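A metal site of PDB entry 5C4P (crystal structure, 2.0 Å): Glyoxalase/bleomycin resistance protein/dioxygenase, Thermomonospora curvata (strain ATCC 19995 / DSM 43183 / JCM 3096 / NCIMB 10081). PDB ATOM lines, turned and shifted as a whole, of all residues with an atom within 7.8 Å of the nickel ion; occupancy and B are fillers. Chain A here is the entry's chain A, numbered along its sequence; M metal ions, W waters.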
ATOM      1  N   GLN A   8      -5.625  21.995 -13.828  1.00  0.00           N
ATOM      2  CA  GLN A   8      -4.708  21.405 -14.824  1.00  0.00           C
ATOM      3  C   GLN A   8      -3.279  21.946 -14.675  1.00  0.00           C
ATOM      4  O   GLN A   8      -3.032  23.125 -14.904  1.00  0.00           O
ATOM      5  CB  GLN A   8      -5.195  21.750 -16.245  1.00  0.00           C
ATOM      6  CG  GLN A   8      -4.400  21.058 -17.344  1.00  0.00           C
ATOM      7  CD  GLN A   8      -4.048  21.972 -18.494  1.00  0.00           C
ATOM      8  OE1 GLN A   8      -4.056  21.541 -19.625  1.00  0.00           O
ATOM      9  NE2 GLN A   8      -3.710  23.237 -18.205  1.00  0.00           N
ATOM     10  N   LEU A   9      -2.330  21.106 -14.254  1.00  0.00           N
ATOM     11  CA  LEU A   9      -0.970  21.585 -14.126  1.00  0.00           C
ATOM     12  C   LEU A   9      -0.146  21.088 -15.346  1.00  0.00           C
ATOM     13  O   LEU A   9       0.102  19.869 -15.453  1.00  0.00           O
ATOM     14  CB  LEU A   9      -0.384  21.048 -12.833  1.00  0.00           C
ATOM     15  CG  LEU A   9       1.097  21.264 -12.678  1.00  0.00           C
ATOM     16  CD1 LEU A   9       1.411  22.767 -12.524  1.00  0.00           C
ATOM     17  CD2 LEU A   9       1.683  20.449 -11.490  1.00  0.00           C
ATOM     18  N   ALA A  10       0.294  21.997 -16.234  1.00  0.00           N
ATOM     19  CA  ALA A  10       1.148  21.527 -17.362  1.00  0.00           C
ATOM     20  C   ALA A  10       2.598  22.020 -17.094  1.00  0.00           C
ATOM     21  O   ALA A  10       2.873  23.236 -17.009  1.00  0.00           O
ATOM     22  CB  ALA A  10       0.617  22.102 -18.657  1.00  0.00           C
ATOM     23  N   TYR A  38       4.880  14.356 -25.151  1.00  0.00           N
ATOM     24  CA  TYR A  38       3.674  14.719 -24.377  1.00  0.00           C
ATOM     25  C   TYR A  38       3.145  13.559 -23.594  1.00  0.00           C
ATOM     26  O   TYR A  38       3.014  12.449 -24.122  1.00  0.00           O
ATOM     27  CB  TYR A  38       2.606  15.230 -25.367  1.00  0.00           C
ATOM     28  CG  TYR A  38       1.324  15.516 -24.715  1.00  0.00           C
ATOM     29  CD1 TYR A  38       0.406  14.485 -24.480  1.00  0.00           C
ATOM     30  CD2 TYR A  38       1.032  16.813 -24.292  1.00  0.00           C
ATOM     31  CE1 TYR A  38      -0.807  14.727 -23.839  1.00  0.00           C
ATOM     32  CE2 TYR A  38      -0.191  17.096 -23.667  1.00  0.00           C
ATOM     33  CZ  TYR A  38      -1.093  16.043 -23.422  1.00  0.00           C
ATOM     34  OH  TYR A  38      -2.291  16.307 -22.800  1.00  0.00           O
ATOM     35  N   LYS A  49      -5.489  17.249 -13.347  1.00  0.00           N
ATOM     36  CA  LYS A  49      -5.053  16.815 -14.658  1.00  0.00           C
ATOM     37  C   LYS A  49      -3.595  17.248 -14.751  1.00  0.00           C
ATOM     38  O   LYS A  49      -3.295  18.467 -14.706  1.00  0.00           O
ATOM     39  CB  LYS A  49      -5.927  17.481 -15.745  1.00  0.00           C
ATOM     40  CG  LYS A  49      -5.435  17.262 -17.189  1.00  0.00           C
ATOM     41  CD  LYS A  49      -5.144  15.789 -17.586  1.00  0.00           C
ATOM     42  CE  LYS A  49      -6.351  14.889 -17.835  1.00  0.00           C
ATOM     43  NZ  LYS A  49      -7.505  15.494 -18.574  1.00  0.00           N
ATOM     44  N   VAL A  51      -0.271  17.466 -16.970  1.00  0.00           N
ATOM     45  CA  VAL A  51       0.239  17.397 -18.321  1.00  0.00           C
ATOM     46  C   VAL A  51       1.749  17.552 -18.279  1.00  0.00           C
ATOM     47  O   VAL A  51       2.297  18.487 -17.646  1.00  0.00           O
ATOM     48  CB  VAL A  51      -0.405  18.507 -19.201  1.00  0.00           C
ATOM     49  CG1 VAL A  51       0.232  18.520 -20.595  1.00  0.00           C
ATOM     50  CG2 VAL A  51      -1.979  18.317 -19.282  1.00  0.00           C
ATOM     51  N   ILE A  53       5.069  18.119 -20.714  1.00  0.00           N
ATOM     52  CA  ILE A  53       5.493  18.461 -22.069  1.00  0.00           C
ATOM     53  C   ILE A  53       6.997  18.489 -22.105  1.00  0.00           C
ATOM     54  O   ILE A  53       7.688  19.131 -21.297  1.00  0.00           O
ATOM     55  CB  ILE A  53       4.969  19.830 -22.515  1.00  0.00           C
ATOM     56  CG1 ILE A  53       3.445  19.822 -22.508  1.00  0.00           C
ATOM     57  CG2 ILE A  53       5.422  20.241 -23.944  1.00  0.00           C
ATOM     58  CD1 ILE A  53       2.884  21.151 -22.131  1.00  0.00           C
ATOM     59  N   ASP A  64       4.552  25.355 -17.699  1.00  0.00           N
ATOM     60  CA  ASP A  64       4.216  25.694 -19.066  1.00  0.00           C
ATOM     61  C   ASP A  64       2.921  26.554 -19.032  1.00  0.00           C
ATOM     62  O   ASP A  64       2.864  27.689 -19.493  1.00  0.00           O
ATOM     63  CB  ASP A  64       3.940  24.361 -19.805  1.00  0.00           C
ATOM     64  CG  ASP A  64       3.740  24.573 -21.335  1.00  0.00           C
ATOM     65  OD1 ASP A  64       4.790  24.580 -22.021  1.00  0.00           O
ATOM     66  OD2 ASP A  64       2.577  24.807 -21.830  1.00  0.00           O
ATOM     67  N   HIS A  65       1.868  26.012 -18.452  1.00  0.00           N
ATOM     68  CA  HIS A  65       0.570  26.741 -18.274  1.00  0.00           C
ATOM     69  C   HIS A  65      -0.293  26.064 -17.214  1.00  0.00           C
ATOM     70  O   HIS A  65       0.075  25.016 -16.701  1.00  0.00           O
ATOM     71  CB  HIS A  65      -0.211  26.942 -19.582  1.00  0.00           C
ATOM     72  CG  HIS A  65      -0.665  25.680 -20.209  1.00  0.00           C
ATOM     73  ND1 HIS A  65       0.178  24.877 -20.962  1.00  0.00           N
ATOM     74  CD2 HIS A  65      -1.880  25.090 -20.241  1.00  0.00           C
ATOM     75  CE1 HIS A  65      -0.505  23.846 -21.420  1.00  0.00           C
ATOM     76  NE2 HIS A  65      -1.745  23.944 -20.976  1.00  0.00           N
ATOM     77  N   LEU A  66      -1.374  26.742 -16.803  1.00  0.00           N
ATOM     78  CA  LEU A  66      -2.242  26.303 -15.746  1.00  0.00           C
ATOM     79  C   LEU A  66      -3.639  26.312 -16.362  1.00  0.00           C
ATOM     80  O   LEU A  66      -3.862  26.867 -17.455  1.00  0.00           O
ATOM     81  CB  LEU A  66      -2.177  27.301 -14.606  1.00  0.00           C
ATOM     82  CG  LEU A  66      -0.827  27.408 -13.893  1.00  0.00           C
ATOM     83  CD1 LEU A  66      -0.595  28.644 -13.006  1.00  0.00           C
ATOM     84  CD2 LEU A  66      -0.667  26.151 -13.067  1.00  0.00           C
ATOM     85  N   GLY A  67      -4.578  25.640 -15.748  1.00  0.00           N
ATOM     86  CA  GLY A  67      -5.943  25.717 -16.280  1.00  0.00           C
ATOM     87  C   GLY A  67      -6.936  25.128 -15.306  1.00  0.00           C
ATOM     88  O   GLY A  67      -6.578  24.646 -14.202  1.00  0.00           O
ATOM     89  N   LYS A 105     -12.939  26.694 -24.983  1.00  0.00           N
ATOM     90  CA  LYS A 105     -11.766  27.183 -24.199  1.00  0.00           C
ATOM     91  C   LYS A 105     -11.785  28.721 -23.988  1.00  0.00           C
ATOM     92  O   LYS A 105     -12.178  29.474 -24.891  1.00  0.00           O
ATOM     93  CB  LYS A 105     -10.459  26.685 -24.891  1.00  0.00           C
ATOM     94  CG  LYS A 105      -9.248  26.639 -23.982  1.00  0.00           C
ATOM     95  CD  LYS A 105      -8.016  25.998 -24.645  1.00  0.00           C
ATOM     96  CE  LYS A 105      -8.061  24.499 -24.665  1.00  0.00           C
ATOM     97  NZ  LYS A 105      -6.693  23.912 -24.648  1.00  0.00           N
ATOM     98  N   TRP A 107      -9.058  31.715 -22.324  1.00  0.00           N
ATOM     99  CA  TRP A 107      -7.732  32.019 -21.781  1.00  0.00           C
ATOM    100  C   TRP A 107      -7.720  33.352 -21.114  1.00  0.00           C
ATOM    101  O   TRP A 107      -8.299  34.328 -21.637  1.00  0.00           O
ATOM    102  CB  TRP A 107      -6.724  32.176 -22.896  1.00  0.00           C
ATOM    103  CG  TRP A 107      -6.410  30.919 -23.576  1.00  0.00           C
ATOM    104  CD1 TRP A 107      -7.023  30.417 -24.689  1.00  0.00           C
ATOM    105  CD2 TRP A 107      -5.426  29.977 -23.177  1.00  0.00           C
ATOM    106  NE1 TRP A 107      -6.415  29.250 -25.058  1.00  0.00           N
ATOM    107  CE2 TRP A 107      -5.452  28.937 -24.120  1.00  0.00           C
ATOM    108  CE3 TRP A 107      -4.493  29.927 -22.102  1.00  0.00           C
ATOM    109  CZ2 TRP A 107      -4.550  27.801 -24.039  1.00  0.00           C
ATOM    110  CZ3 TRP A 107      -3.632  28.795 -21.968  1.00  0.00           C
ATOM    111  CH2 TRP A 107      -3.631  27.768 -22.953  1.00  0.00           C
ATOM    112  N   GLU A 117      -6.052  28.498 -18.808  1.00  0.00           N
ATOM    113  CA  GLU A 117      -7.111  28.087 -19.735  1.00  0.00           C
ATOM    114  C   GLU A 117      -8.274  27.488 -18.933  1.00  0.00           C
ATOM    115  O   GLU A 117      -8.055  26.708 -17.995  1.00  0.00           O
ATOM    116  CB  GLU A 117      -6.587  27.057 -20.700  1.00  0.00           C
ATOM    117  CG  GLU A 117      -5.896  25.856 -20.102  1.00  0.00           C
ATOM    118  CD  GLU A 117      -5.426  24.929 -21.178  1.00  0.00           C
ATOM    119  OE1 GLU A 117      -5.811  25.171 -22.322  1.00  0.00           O
ATOM    120  OE2 GLU A 117      -4.659  23.978 -20.915  1.00  0.00           O
ATOM    121  N   TYR A 119     -11.373  25.055 -19.732  1.00  0.00           N
ATOM    122  CA  TYR A 119     -11.565  24.252 -20.917  1.00  0.00           C
ATOM    123  C   TYR A 119     -12.335  23.027 -20.538  1.00  0.00           C
ATOM    124  O   TYR A 119     -12.366  22.636 -19.383  1.00  0.00           O
ATOM    125  CB  TYR A 119     -10.194  23.884 -21.621  1.00  0.00           C
ATOM    126  CG  TYR A 119      -9.418  22.847 -20.846  1.00  0.00           C
ATOM    127  CD1 TYR A 119      -8.640  23.244 -19.750  1.00  0.00           C
ATOM    128  CD2 TYR A 119      -9.515  21.469 -21.140  1.00  0.00           C
ATOM    129  CE1 TYR A 119      -7.988  22.304 -18.948  1.00  0.00           C
ATOM    130  CE2 TYR A 119      -8.831  20.512 -20.365  1.00  0.00           C
ATOM    131  CZ  TYR A 119      -8.072  20.947 -19.271  1.00  0.00           C
ATOM    132  OH  TYR A 119      -7.410  20.037 -18.425  1.00  0.00           O
HETATM  133 NI    NI M   1      -3.432  22.628 -21.427  1.00  0.00          NI
HETATM  134  O   HOH W   1      -5.371  21.610 -22.066  1.00  0.00           O
HETATM  135  O   HOH W   2      -2.266  21.088 -22.064  1.00  0.00           O
HETATM  136  O   HOH W   3      -3.515  23.627 -23.411  1.00  0.00           O
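The nickel ion is bound by the side-chain carboxylate (OE2) of Glu 117, water W2, a ring nitrogen (NE2) of His 65, the side-chain amide oxygen (OE1) of Gln 8, water W3 and water W1.
Water W3 lies within hydrogen-bond range of OE1 of Glu 117 (3.0 Å) and NZ of Lys 105 (3.4 Å).
Within 4 Å of the nickel ion: Gln 8, His 65 and Glu 117.
The side-chain carboxylate of Glu 117 lies within salt-bridge range of the side-chain amino group of Lys 105 (2.8 Å).
The backbone NH (N) of Glu 117 sits at hydrogen-bond distance from the backbone carbonyl oxygen (O) of Leu 66 (3.0 Å).
The backbone carbonyl oxygen (O) of His 65 sits at hydrogen-bond distance from the backbone NH (N) of Ala 10 (3.1 Å).
A ring nitrogen (ND1) of His 65 is in hydrogen-bond range of the side-chain carboxylate (OD2) of Asp 64.
The backbone NH of Gln 8 lies within hydrogen-bond range of the backbone carbonyl oxygen of Gly 67, 2.8 Å away.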
